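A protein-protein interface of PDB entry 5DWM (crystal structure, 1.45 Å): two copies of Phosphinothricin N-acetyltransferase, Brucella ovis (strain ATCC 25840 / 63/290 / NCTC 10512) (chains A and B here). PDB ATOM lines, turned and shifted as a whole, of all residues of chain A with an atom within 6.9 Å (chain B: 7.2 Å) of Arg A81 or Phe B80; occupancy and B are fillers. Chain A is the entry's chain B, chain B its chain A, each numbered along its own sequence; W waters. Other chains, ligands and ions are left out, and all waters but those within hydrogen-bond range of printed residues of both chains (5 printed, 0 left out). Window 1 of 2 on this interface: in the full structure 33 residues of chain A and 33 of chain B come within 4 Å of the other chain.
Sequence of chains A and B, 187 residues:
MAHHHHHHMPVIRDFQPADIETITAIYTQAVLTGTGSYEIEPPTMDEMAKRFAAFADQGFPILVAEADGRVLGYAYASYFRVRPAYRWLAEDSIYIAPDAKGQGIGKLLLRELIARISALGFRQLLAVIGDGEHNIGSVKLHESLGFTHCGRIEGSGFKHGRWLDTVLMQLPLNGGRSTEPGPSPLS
N of Ala A85 sits at hydrogen-bond distance from O of Tyr B38 (3.0 Å).
OE1 of Glu B91 lies within salt-bridge range of NH2 of Arg A81 (2.6 Å).
NH2 of Arg B81 is in salt-bridge range of OE1 of Glu A91 (2.6 Å).
The backbone carbonyl oxygen (O) of Phe A80 sits close to the guanidinium group (NH2) of Arg B81.
O of Ser B78 sits at hydrogen-bond distance from N of Glu B91, 2.7 Å away.
The side-chain hydroxyl (OG) of Ser A156 is in hydrogen-bond range of the side-chain hydroxyl (OG1) of Thr A166, 2.6 Å away.
The side-chain hydroxyl (OH) of Tyr B38 is in hydrogen-bond range of the side-chain hydroxyl (OG1) of Thr B166 (3.5 Å).
The backbone NH (N) of Glu A91 sits at hydrogen-bond distance from the backbone carbonyl oxygen (O) of Ser A78 (2.8 Å).
Among the printed residues, pairs that only touch across the chains: Arg A81 with Phe B80, Leu A168 with Leu B168, Tyr A86 with Tyr B38, Ser A156 with Tyr B86, Pro A84 with Tyr B38, Arg A83 with Tyr B38, Arg A81 with Val B128, Val A128 with Arg B81 and Ser A156 with Leu B89.
Arg A81 touches just these residues of chain B: Phe B80, Glu B91 and Val B128.
Phe B80 touches just one residue of chain A: Arg A81 (3.1 Å).
Printed residues of chain A within 4 Å of Leu B89: Ser A156 (3.9 Å).
Ala B90 touches none of the printed residues of chain A.
Printed residues of chain A within 4 Å of Glu B91: Arg A81 (2.6 Å).
The nearest residue of chain B that does not touch Arg A81 is Tyr B79 (5.0 Å).
The nearest printed residue of chain B that does not touch Tyr A86 is Val B128 (4.1 Å).
Printed residues of chain B that touch a printed residue of chain A: Tyr B38, Phe B80, Arg B81, Tyr B86, Leu B89, Glu B91, Val B128 and Leu B168.
Hydrophobic or aromatic side chains of chain B within 4 Å of the printed part of chain A: Tyr B38, Phe B80, Tyr B86, Leu B89, Val B128 and Leu B168.
Printed residues of chain A that touch a printed residue of chain B: Phe A80, Arg A81, Arg A83, Pro A84, Ala A85, Tyr A86, Glu A91, Val A128, Ser A156 and Leu A168.
Among the printed residues, 13 pairs touch across the chains.
Phe A80 touches Arg B81, and with the chains exchanged Arg A81 touches Phe B80.
Arg A81 touches Glu B91, and with the chains exchanged Glu A91 touches Arg B81.
Arg A81 touches Val B128, and with the chains exchanged Val A128 touches Arg B81.
Leu B168 touches its own counterpart, Leu A168.
Water W1 bridges NE of Arg B81 (2.7 Å) and O of Phe A80 (2.9 Å).
Water W5 lies within hydrogen-bond range of the backbone carbonyl oxygen (O) of Tyr A79 (2.7 Å), the side-chain carboxylate (OE1) of Glu A91 (3.0 Å) and the guanidinium group (NH2) of Arg B81 (3.5 Å).
Water W3 bridges OG1 of Thr B166 (2.7 Å) and OH of Tyr A86 (2.7 Å).
Water W4 bridges the side-chain hydroxyl (OH) of Tyr B86 (2.7 Å) and the side-chain hydroxyl (OG1) of Thr A166 (2.7 Å).
Water W2 bridges the backbone carbonyl oxygen (O) of Ser A156 (3.0 Å) and the backbone carbonyl oxygen (O) of Tyr B86 (3.4 Å).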
ATOM      1  N   SER A  78     -18.932   0.590  14.071  1.00  0.00           N
ATOM      2  CA  SER A  78     -18.597   0.713  15.484  1.00  0.00           C
ATOM      3  C   SER A  78     -18.670   2.192  15.836  1.00  0.00           C
ATOM      4  O   SER A  78     -18.971   3.029  14.983  1.00  0.00           O
ATOM      5  CB  SER A  78     -17.217   0.117  15.774  1.00  0.00           C
ATOM      6  OG  SER A  78     -16.235   0.772  15.000  1.00  0.00           O
ATOM      7  N   TYR A  79     -18.396   2.517  17.096  1.00  0.00           N
ATOM      8  CA  TYR A  79     -18.379   3.918  17.491  1.00  0.00           C
ATOM      9  C   TYR A  79     -17.090   4.572  17.024  1.00  0.00           C
ATOM     10  O   TYR A  79     -16.018   3.958  17.060  1.00  0.00           O
ATOM     11  CB  TYR A  79     -18.488   4.079  19.009  1.00  0.00           C
ATOM     12  CG  TYR A  79     -19.859   3.780  19.562  1.00  0.00           C
ATOM     13  CD1 TYR A  79     -20.975   4.512  19.158  1.00  0.00           C
ATOM     14  CD2 TYR A  79     -20.041   2.774  20.503  1.00  0.00           C
ATOM     15  CE1 TYR A  79     -22.241   4.229  19.672  1.00  0.00           C
ATOM     16  CE2 TYR A  79     -21.296   2.483  21.017  1.00  0.00           C
ATOM     17  CZ  TYR A  79     -22.395   3.216  20.601  1.00  0.00           C
ATOM     18  OH  TYR A  79     -23.640   2.928  21.114  1.00  0.00           O
ATOM     19  N   PHE A  80     -17.206   5.824  16.577  1.00  0.00           N
ATOM     20  CA  PHE A  80     -16.025   6.662  16.421  1.00  0.00           C
ATOM     21  C   PHE A  80     -15.386   6.938  17.781  1.00  0.00           C
ATOM     22  O   PHE A  80     -14.194   6.671  17.990  1.00  0.00           O
ATOM     23  CB  PHE A  80     -16.424   7.971  15.736  1.00  0.00           C
ATOM     24  CG  PHE A  80     -15.363   9.036  15.796  1.00  0.00           C
ATOM     25  CD1 PHE A  80     -14.191   8.902  15.075  1.00  0.00           C
ATOM     26  CD2 PHE A  80     -15.550  10.172  16.572  1.00  0.00           C
ATOM     27  CE1 PHE A  80     -13.219   9.880  15.125  1.00  0.00           C
ATOM     28  CE2 PHE A  80     -14.580  11.155  16.633  1.00  0.00           C
ATOM     29  CZ  PHE A  80     -13.410  11.011  15.912  1.00  0.00           C
ATOM     30  N   ARG A  81     -16.179   7.470  18.720  1.00  0.00           N
ATOM     31  CA  ARG A  81     -15.807   7.661  20.116  1.00  0.00           C
ATOM     32  C   ARG A  81     -17.016   7.326  20.982  1.00  0.00           C
ATOM     33  O   ARG A  81     -18.154   7.332  20.512  1.00  0.00           O
ATOM     34  CB  ARG A  81     -15.291   9.084  20.364  1.00  0.00           C
ATOM     35  CG  ARG A  81     -13.919   9.274  19.748  1.00  0.00           C
ATOM     36  CD  ARG A  81     -13.274  10.589  20.051  1.00  0.00           C
ATOM     37  NE  ARG A  81     -11.887  10.530  19.614  1.00  0.00           N
ATOM     38  CZ  ARG A  81     -10.961  11.436  19.904  1.00  0.00           C
ATOM     39  NH1 ARG A  81     -11.265  12.498  20.636  1.00  0.00           N
ATOM     40  NH2 ARG A  81      -9.729  11.274  19.457  1.00  0.00           N
ATOM     41  N   VAL A  82     -16.765   6.992  22.250  1.00  0.00           N
ATOM     42  CA  VAL A  82     -17.793   6.361  23.077  1.00  0.00           C
ATOM     43  C   VAL A  82     -18.523   7.308  24.024  1.00  0.00           C
ATOM     44  O   VAL A  82     -19.521   6.888  24.631  1.00  0.00           O
ATOM     45  CB  VAL A  82     -17.257   5.129  23.837  1.00  0.00           C
ATOM     46  CG1 VAL A  82     -16.698   4.114  22.856  1.00  0.00           C
ATOM     47  CG2 VAL A  82     -16.207   5.554  24.857  1.00  0.00           C
ATOM     48  N   ARG A  83     -18.069   8.553  24.187  1.00  0.00           N
ATOM     49  CA  ARG A  83     -18.767   9.448  25.104  1.00  0.00           C
ATOM     50  C   ARG A  83     -20.207   9.663  24.622  1.00  0.00           C
ATOM     51  O   ARG A  83     -20.482   9.608  23.415  1.00  0.00           O
ATOM     52  CB  ARG A  83     -18.040  10.791  25.248  1.00  0.00           C
ATOM     53  CG  ARG A  83     -16.625  10.759  25.858  1.00  0.00           C
ATOM     54  CD  ARG A  83     -16.503   9.881  27.083  1.00  0.00           C
ATOM     55  NE  ARG A  83     -15.155   9.966  27.652  1.00  0.00           N
ATOM     56  CZ  ARG A  83     -14.643   9.080  28.502  1.00  0.00           C
ATOM     57  NH1 ARG A  83     -15.364   8.030  28.876  1.00  0.00           N
ATOM     58  NH2 ARG A  83     -13.409   9.231  28.970  1.00  0.00           N
ATOM     59  N   PRO A  84     -21.153   9.892  25.545  1.00  0.00           N
ATOM     60  CA  PRO A  84     -22.581   9.775  25.180  1.00  0.00           C
ATOM     61  C   PRO A  84     -23.073  10.719  24.090  1.00  0.00           C
ATOM     62  O   PRO A  84     -23.990  10.349  23.350  1.00  0.00           O
ATOM     63  CB  PRO A  84     -23.310  10.012  26.509  1.00  0.00           C
ATOM     64  CG  PRO A  84     -22.317   9.609  27.554  1.00  0.00           C
ATOM     65  CD  PRO A  84     -20.961   9.967  27.005  1.00  0.00           C
ATOM     66  N   ALA A  85     -22.535  11.933  23.969  1.00  0.00           N
ATOM     67  CA  ALA A  85     -23.053  12.813  22.925  1.00  0.00           C
ATOM     68  C   ALA A  85     -22.772  12.288  21.524  1.00  0.00           C
ATOM     69  O   ALA A  85     -23.451  12.699  20.582  1.00  0.00           O
ATOM     70  CB  ALA A  85     -22.560  14.255  23.095  1.00  0.00           C
ATOM     71  N   TYR A  86     -21.809  11.375  21.380  1.00  0.00           N
ATOM     72  CA  TYR A  86     -21.441  10.774  20.101  1.00  0.00           C
ATOM     73  C   TYR A  86     -22.314   9.583  19.721  1.00  0.00           C
ATOM     74  O   TYR A  86     -22.018   8.935  18.715  1.00  0.00           O
ATOM     75  CB  TYR A  86     -20.014  10.224  20.180  1.00  0.00           C
ATOM     76  CG  TYR A  86     -18.862  11.204  20.127  1.00  0.00           C
ATOM     77  CD1 TYR A  86     -18.568  11.911  18.961  1.00  0.00           C
ATOM     78  CD2 TYR A  86     -17.996  11.339  21.213  1.00  0.00           C
ATOM     79  CE1 TYR A  86     -17.471  12.759  18.891  1.00  0.00           C
ATOM     80  CE2 TYR A  86     -16.888  12.185  21.147  1.00  0.00           C
ATOM     81  CZ  TYR A  86     -16.635  12.889  19.978  1.00  0.00           C
ATOM     82  OH  TYR A  86     -15.543  13.726  19.903  1.00  0.00           O
ATOM     83  N   ARG A  87     -23.368   9.264  20.473  1.00  0.00           N
ATOM     84  CA  ARG A  87     -24.051   7.983  20.314  1.00  0.00           C
ATOM     85  C   ARG A  87     -24.876   7.878  19.037  1.00  0.00           C
ATOM     86  O   ARG A  87     -25.369   6.784  18.731  1.00  0.00           O
ATOM     87  CB  ARG A  87     -24.921   7.685  21.537  1.00  0.00           C
ATOM     88  CG  ARG A  87     -24.155   7.081  22.704  1.00  0.00           C
ATOM     89  CD  ARG A  87     -25.084   6.696  23.849  1.00  0.00           C
ATOM     90  NE  ARG A  87     -25.893   5.517  23.538  1.00  0.00           N
ATOM     91  CZ  ARG A  87     -25.555   4.271  23.853  1.00  0.00           C
ATOM     92  NH1 ARG A  87     -24.420   4.032  24.495  1.00  0.00           N
ATOM     93  NH2 ARG A  87     -26.353   3.262  23.526  1.00  0.00           N
ATOM     94  N   LEU A  89     -23.427   8.720  16.134  1.00  0.00           N
ATOM     95  CA  LEU A  89     -22.367   8.686  15.129  1.00  0.00           C
ATOM     96  C   LEU A  89     -21.764   7.292  15.096  1.00  0.00           C
ATOM     97  O   LEU A  89     -21.325   6.779  16.134  1.00  0.00           O
ATOM     98  CB  LEU A  89     -21.277   9.707  15.470  1.00  0.00           C
ATOM     99  CG  LEU A  89     -20.006   9.730  14.620  1.00  0.00           C
ATOM    100  CD1 LEU A  89     -20.328  10.170  13.218  1.00  0.00           C
ATOM    101  CD2 LEU A  89     -18.979  10.666  15.259  1.00  0.00           C
ATOM    102  N   GLU A  91     -19.026   4.604  12.728  1.00  0.00           N
ATOM    103  CA  GLU A  91     -17.892   4.572  11.815  1.00  0.00           C
ATOM    104  C   GLU A  91     -17.903   3.252  11.060  1.00  0.00           C
ATOM    105  O   GLU A  91     -18.160   2.198  11.656  1.00  0.00           O
ATOM    106  CB  GLU A  91     -16.594   4.679  12.616  1.00  0.00           C
ATOM    107  CG  GLU A  91     -15.341   4.529  11.792  1.00  0.00           C
ATOM    108  CD  GLU A  91     -14.076   4.755  12.598  1.00  0.00           C
ATOM    109  OE1 GLU A  91     -14.153   5.347  13.695  1.00  0.00           O
ATOM    110  OE2 GLU A  91     -13.001   4.354  12.116  1.00  0.00           O
ATOM    111  N   VAL A 128     -13.091   6.742   8.242  1.00  0.00           N
ATOM    112  CA  VAL A 128     -11.763   7.205   8.636  1.00  0.00           C
ATOM    113  C   VAL A 128     -10.791   6.410   7.771  1.00  0.00           C
ATOM    114  O   VAL A 128     -10.428   5.272   8.105  1.00  0.00           O
ATOM    115  CB  VAL A 128     -11.528   6.972  10.142  1.00  0.00           C
ATOM    116  CG1 VAL A 128     -10.137   7.459  10.570  1.00  0.00           C
ATOM    117  CG2 VAL A 128     -12.625   7.659  10.980  1.00  0.00           C
ATOM    118  N   ILE A 153      -6.455  14.541   8.068  1.00  0.00           N
ATOM    119  CA  ILE A 153      -5.395  14.704   9.062  1.00  0.00           C
ATOM    120  C   ILE A 153      -4.099  14.309   8.367  1.00  0.00           C
ATOM    121  O   ILE A 153      -3.883  13.127   8.073  1.00  0.00           O
ATOM    122  CB  ILE A 153      -5.634  13.845  10.310  1.00  0.00           C
ATOM    123  CG1 ILE A 153      -7.023  14.098  10.900  1.00  0.00           C
ATOM    124  CG2 ILE A 153      -4.536  14.091  11.359  1.00  0.00           C
ATOM    125  CD1 ILE A 153      -7.421  13.102  11.972  1.00  0.00           C
ATOM    126  N   SER A 156      -0.830  11.505   9.738  1.00  0.00           N
ATOM    127  CA  SER A 156      -1.372  10.828  10.905  1.00  0.00           C
ATOM    128  C   SER A 156      -0.722   9.471  11.150  1.00  0.00           C
ATOM    129  O   SER A 156      -0.747   8.981  12.286  1.00  0.00           O
ATOM    130  CB  SER A 156      -2.873  10.628  10.706  1.00  0.00           C
ATOM    131  OG  SER A 156      -3.088   9.792   9.573  1.00  0.00           O
ATOM    132  N   THR A 166      -4.897  10.690   6.852  1.00  0.00           N
ATOM    133  CA  THR A 166      -6.220  10.127   7.099  1.00  0.00           C
ATOM    134  C   THR A 166      -7.255  11.005   6.415  1.00  0.00           C
ATOM    135  O   THR A 166      -7.340  12.199   6.702  1.00  0.00           O
ATOM    136  CB  THR A 166      -6.513  10.093   8.597  1.00  0.00           C
ATOM    137  OG1 THR A 166      -5.604   9.198   9.239  1.00  0.00           O
ATOM    138  CG2 THR A 166      -7.968   9.662   8.851  1.00  0.00           C
ATOM    139  N   LEU A 168     -11.149  11.827   5.996  1.00  0.00           N
ATOM    140  CA  LEU A 168     -12.415  11.658   6.696  1.00  0.00           C
ATOM    141  C   LEU A 168     -13.569  11.989   5.762  1.00  0.00           C
ATOM    142  O   LEU A 168     -13.519  12.984   5.035  1.00  0.00           O
ATOM    143  CB  LEU A 168     -12.474  12.589   7.905  1.00  0.00           C
ATOM    144  CG  LEU A 168     -11.323  12.397   8.890  1.00  0.00           C
ATOM    145  CD1 LEU A 168     -11.178  13.622   9.742  1.00  0.00           C
ATOM    146  CD2 LEU A 168     -11.571  11.181   9.740  1.00  0.00           C
ATOM    147  N   TYR B  38     -18.137  16.049  25.301  1.00  0.00           N
ATOM    148  CA  TYR B  38     -19.275  15.249  24.874  1.00  0.00           C
ATOM    149  C   TYR B  38     -19.757  14.288  25.956  1.00  0.00           C
ATOM    150  O   TYR B  38     -20.568  13.398  25.667  1.00  0.00           O
ATOM    151  CB  TYR B  38     -18.983  14.515  23.560  1.00  0.00           C
ATOM    152  CG  TYR B  38     -19.092  15.372  22.312  1.00  0.00           C
ATOM    153  CD1 TYR B  38     -19.031  16.771  22.370  1.00  0.00           C
ATOM    154  CD2 TYR B  38     -19.270  14.778  21.063  1.00  0.00           C
ATOM    155  CE1 TYR B  38     -19.133  17.546  21.205  1.00  0.00           C
ATOM    156  CE2 TYR B  38     -19.374  15.536  19.908  1.00  0.00           C
ATOM    157  CZ  TYR B  38     -19.292  16.911  19.977  1.00  0.00           C
ATOM    158  OH  TYR B  38     -19.394  17.657  18.814  1.00  0.00           O
ATOM    159  N   PHE B  60       2.458  10.445  29.044  1.00  0.00           N
ATOM    160  CA  PHE B  60       2.024  11.729  28.522  1.00  0.00           C
ATOM    161  C   PHE B  60       2.125  12.813  29.590  1.00  0.00           C
ATOM    162  O   PHE B  60       1.927  12.544  30.778  1.00  0.00           O
ATOM    163  CB  PHE B  60       0.576  11.642  28.044  1.00  0.00           C
ATOM    164  CG  PHE B  60       0.418  10.905  26.739  1.00  0.00           C
ATOM    165  CD1 PHE B  60       0.843  11.482  25.557  1.00  0.00           C
ATOM    166  CD2 PHE B  60      -0.155   9.643  26.694  1.00  0.00           C
ATOM    167  CE1 PHE B  60       0.718  10.809  24.345  1.00  0.00           C
ATOM    168  CE2 PHE B  60      -0.291   8.961  25.480  1.00  0.00           C
ATOM    169  CZ  PHE B  60       0.146   9.553  24.306  1.00  0.00           C
ATOM    170  N   SER B  78      -2.691  12.865  24.871  1.00  0.00           N
ATOM    171  CA  SER B  78      -2.960  11.429  24.822  1.00  0.00           C
ATOM    172  C   SER B  78      -2.944  11.012  23.356  1.00  0.00           C
ATOM    173  O   SER B  78      -2.753  11.839  22.464  1.00  0.00           O
ATOM    174  CB  SER B  78      -4.298  11.096  25.493  1.00  0.00           C
ATOM    175  OG  SER B  78      -5.365  11.785  24.856  1.00  0.00           O
ATOM    176  N   TYR B  79      -3.159   9.725  23.100  1.00  0.00           N
ATOM    177  CA  TYR B  79      -3.261   9.276  21.719  1.00  0.00           C
ATOM    178  C   TYR B  79      -4.610   9.657  21.125  1.00  0.00           C
ATOM    179  O   TYR B  79      -5.637   9.644  21.814  1.00  0.00           O
ATOM    180  CB  TYR B  79      -3.064   7.760  21.606  1.00  0.00           C
ATOM    181  CG  TYR B  79      -1.645   7.322  21.856  1.00  0.00           C
ATOM    182  CD1 TYR B  79      -0.611   7.748  21.027  1.00  0.00           C
ATOM    183  CD2 TYR B  79      -1.337   6.480  22.917  1.00  0.00           C
ATOM    184  CE1 TYR B  79       0.695   7.355  21.263  1.00  0.00           C
ATOM    185  CE2 TYR B  79      -0.043   6.086  23.163  1.00  0.00           C
ATOM    186  CZ  TYR B  79       0.970   6.522  22.334  1.00  0.00           C
ATOM    187  OH  TYR B  79       2.254   6.117  22.582  1.00  0.00           O
ATOM    188  N   PHE B  80      -4.598  10.000  19.834  1.00  0.00           N
ATOM    189  CA  PHE B  80      -5.841  10.049  19.065  1.00  0.00           C
ATOM    190  C   PHE B  80      -6.425   8.649  18.921  1.00  0.00           C
ATOM    191  O   PHE B  80      -7.583   8.400  19.290  1.00  0.00           O
ATOM    192  CB  PHE B  80      -5.579  10.679  17.691  1.00  0.00           C
ATOM    193  CG  PHE B  80      -6.708  10.513  16.718  1.00  0.00           C
ATOM    194  CD1 PHE B  80      -7.913  11.157  16.913  1.00  0.00           C
ATOM    195  CD2 PHE B  80      -6.562   9.696  15.599  1.00  0.00           C
ATOM    196  CE1 PHE B  80      -8.963  10.991  16.006  1.00  0.00           C
ATOM    197  CE2 PHE B  80      -7.597   9.523  14.694  1.00  0.00           C
ATOM    198  CZ  PHE B  80      -8.801  10.172  14.897  1.00  0.00           C
ATOM    199  N   ARG B  81      -5.622   7.725  18.395  1.00  0.00           N
ATOM    200  CA  ARG B  81      -5.919   6.301  18.328  1.00  0.00           C
ATOM    201  C   ARG B  81      -4.628   5.538  18.610  1.00  0.00           C
ATOM    202  O   ARG B  81      -3.528   6.073  18.454  1.00  0.00           O
ATOM    203  CB  ARG B  81      -6.511   5.939  16.962  1.00  0.00           C
ATOM    204  CG  ARG B  81      -7.910   6.494  16.825  1.00  0.00           C
ATOM    205  CD  ARG B  81      -8.640   6.059  15.581  1.00  0.00           C
ATOM    206  NE  ARG B  81     -10.053   6.376  15.740  1.00  0.00           N
ATOM    207  CZ  ARG B  81     -11.008   6.022  14.890  1.00  0.00           C
ATOM    208  NH1 ARG B  81     -10.700   5.346  13.794  1.00  0.00           N
ATOM    209  NH2 ARG B  81     -12.269   6.355  15.137  1.00  0.00           N
ATOM    210  N   VAL B  82      -4.761   4.276  19.032  1.00  0.00           N
ATOM    211  CA  VAL B  82      -3.636   3.571  19.649  1.00  0.00           C
ATOM    212  C   VAL B  82      -2.879   2.625  18.719  1.00  0.00           C
ATOM    213  O   VAL B  82      -1.819   2.114  19.114  1.00  0.00           O
ATOM    214  CB  VAL B  82      -4.042   2.843  20.946  1.00  0.00           C
ATOM    215  CG1 VAL B  82      -4.606   3.847  21.969  1.00  0.00           C
ATOM    216  CG2 VAL B  82      -5.033   1.737  20.631  1.00  0.00           C
ATOM    217  N   ARG B  83      -3.359   2.376  17.508  1.00  0.00           N
ATOM    218  CA  ARG B  83      -2.671   1.441  16.626  1.00  0.00           C
ATOM    219  C   ARG B  83      -1.280   1.979  16.267  1.00  0.00           C
ATOM    220  O   ARG B  83      -1.075   3.194  16.203  1.00  0.00           O
ATOM    221  CB  ARG B  83      -3.486   1.179  15.357  1.00  0.00           C
ATOM    222  CG  ARG B  83      -4.882   0.577  15.593  1.00  0.00           C
ATOM    223  CD  ARG B  83      -4.858  -0.629  16.536  1.00  0.00           C
ATOM    224  NE  ARG B  83      -6.179  -1.251  16.645  1.00  0.00           N
ATOM    225  CZ  ARG B  83      -6.521  -2.147  17.568  1.00  0.00           C
ATOM    226  NH1 ARG B  83      -5.644  -2.541  18.478  1.00  0.00           N
ATOM    227  NH2 ARG B  83      -7.748  -2.645  17.585  1.00  0.00           N
ATOM    228  N   TYR B  86      -0.087   5.168  14.251  1.00  0.00           N
ATOM    229  CA  TYR B  86      -0.502   6.448  14.825  1.00  0.00           C
ATOM    230  C   TYR B  86       0.435   6.963  15.921  1.00  0.00           C
ATOM    231  O   TYR B  86       0.139   8.005  16.518  1.00  0.00           O
ATOM    232  CB  TYR B  86      -1.884   6.310  15.474  1.00  0.00           C
ATOM    233  CG  TYR B  86      -3.100   6.282  14.564  1.00  0.00           C
ATOM    234  CD1 TYR B  86      -3.452   7.388  13.795  1.00  0.00           C
ATOM    235  CD2 TYR B  86      -3.947   5.173  14.535  1.00  0.00           C
ATOM    236  CE1 TYR B  86      -4.597   7.382  13.003  1.00  0.00           C
ATOM    237  CE2 TYR B  86      -5.093   5.160  13.742  1.00  0.00           C
ATOM    238  CZ  TYR B  86      -5.415   6.266  12.978  1.00  0.00           C
ATOM    239  OH  TYR B  86      -6.566   6.251  12.205  1.00  0.00           O
ATOM    240  N   LEU B  89       1.367  10.676  16.525  1.00  0.00           N
ATOM    241  CA  LEU B  89       0.239  11.597  16.555  1.00  0.00           C
ATOM    242  C   LEU B  89      -0.271  11.662  17.990  1.00  0.00           C
ATOM    243  O   LEU B  89      -0.600  10.628  18.580  1.00  0.00           O
ATOM    244  CB  LEU B  89      -0.861  11.088  15.615  1.00  0.00           C
ATOM    245  CG  LEU B  89      -2.197  11.845  15.664  1.00  0.00           C
ATOM    246  CD1 LEU B  89      -2.001  13.265  15.150  1.00  0.00           C
ATOM    247  CD2 LEU B  89      -3.254  11.090  14.855  1.00  0.00           C
ATOM    248  N   ALA B  90      -0.287  12.864  18.572  1.00  0.00           N
ATOM    249  CA  ALA B  90      -0.877  13.080  19.884  1.00  0.00           C
ATOM    250  C   ALA B  90      -2.075  14.016  19.761  1.00  0.00           C
ATOM    251  O   ALA B  90      -2.215  14.747  18.780  1.00  0.00           O
ATOM    252  CB  ALA B  90       0.142  13.665  20.871  1.00  0.00           C
ATOM    253  N   GLU B  91      -2.936  13.990  20.778  1.00  0.00           N
ATOM    254  CA  GLU B  91      -4.118  14.838  20.845  1.00  0.00           C
ATOM    255  C   GLU B  91      -4.067  15.664  22.125  1.00  0.00           C
ATOM    256  O   GLU B  91      -3.698  15.144  23.181  1.00  0.00           O
ATOM    257  CB  GLU B  91      -5.381  13.962  20.843  1.00  0.00           C
ATOM    258  CG  GLU B  91      -6.685  14.751  20.887  1.00  0.00           C
ATOM    259  CD  GLU B  91      -7.906  13.851  20.862  1.00  0.00           C
ATOM    260  OE1 GLU B  91      -7.812  12.731  20.323  1.00  0.00           O
ATOM    261  OE2 GLU B  91      -8.956  14.271  21.378  1.00  0.00           O
ATOM    262  N   SER B  93      -5.863  18.247  25.093  1.00  0.00           N
ATOM    263  CA  SER B  93      -7.094  18.504  25.833  1.00  0.00           C
ATOM    264  C   SER B  93      -6.819  19.618  26.829  1.00  0.00           C
ATOM    265  O   SER B  93      -5.827  19.555  27.557  1.00  0.00           O
ATOM    266  CB  SER B  93      -7.520  17.254  26.604  1.00  0.00           C
ATOM    267  OG  SER B  93      -7.873  16.218  25.708  1.00  0.00           O
ATOM    268  N   LEU B 126      -2.960  17.047  17.519  1.00  0.00           N
ATOM    269  CA  LEU B 126      -4.313  17.172  16.988  1.00  0.00           C
ATOM    270  C   LEU B 126      -5.248  17.722  18.058  1.00  0.00           C
ATOM    271  O   LEU B 126      -5.226  17.258  19.200  1.00  0.00           O
ATOM    272  CB  LEU B 126      -4.816  15.792  16.553  1.00  0.00           C
ATOM    273  CG  LEU B 126      -6.215  15.709  15.928  1.00  0.00           C
ATOM    274  CD1 LEU B 126      -6.208  16.291  14.522  1.00  0.00           C
ATOM    275  CD2 LEU B 126      -6.718  14.266  15.903  1.00  0.00           C
ATOM    276  N   VAL B 128      -9.285  18.014  18.820  1.00  0.00           N
ATOM    277  CA  VAL B 128     -10.604  17.511  18.455  1.00  0.00           C
ATOM    278  C   VAL B 128     -11.588  18.356  19.252  1.00  0.00           C
ATOM    279  O   VAL B 128     -11.855  18.076  20.426  1.00  0.00           O
ATOM    280  CB  VAL B 128     -10.726  16.014  18.798  1.00  0.00           C
ATOM    281  CG1 VAL B 128     -12.103  15.480  18.399  1.00  0.00           C
ATOM    282  CG2 VAL B 128      -9.649  15.223  18.088  1.00  0.00           C
ATOM    283  N   THR B 166     -17.795  18.639  15.303  1.00  0.00           N
ATOM    284  CA  THR B 166     -16.427  18.496  15.797  1.00  0.00           C
ATOM    285  C   THR B 166     -15.489  19.191  14.821  1.00  0.00           C
ATOM    286  O   THR B 166     -15.428  18.811  13.649  1.00  0.00           O
ATOM    287  CB  THR B 166     -16.040  17.024  15.867  1.00  0.00           C
ATOM    288  OG1 THR B 166     -16.878  16.344  16.800  1.00  0.00           O
ATOM    289  CG2 THR B 166     -14.572  16.881  16.285  1.00  0.00           C
ATOM    290  N   LEU B 168     -11.696  19.820  13.716  1.00  0.00           N
ATOM    291  CA  LEU B 168     -10.372  19.222  13.846  1.00  0.00           C
ATOM    292  C   LEU B 168      -9.302  20.214  13.403  1.00  0.00           C
ATOM    293  O   LEU B 168      -9.452  20.879  12.371  1.00  0.00           O
ATOM    294  CB  LEU B 168     -10.259  17.957  12.991  1.00  0.00           C
ATOM    295  CG  LEU B 168     -11.343  16.916  13.251  1.00  0.00           C
ATOM    296  CD1 LEU B 168     -11.332  15.944  12.117  1.00  0.00           C
ATOM    297  CD2 LEU B 168     -11.077  16.204  14.551  1.00  0.00           C
HETATM  298  O   HOH W   1     -11.432   7.454  17.746  1.00  0.00           O
HETATM  299  O   HOH W   2       1.910   8.643  13.681  1.00  0.00           O
HETATM  300  O   HOH W   3     -15.950  16.369  19.301  1.00  0.00           O
HETATM  301  O   HOH W   4      -6.510   6.640   9.519  1.00  0.00           O
HETATM  302  O   HOH W   5     -13.742   3.278  15.850  1.00  0.00           O
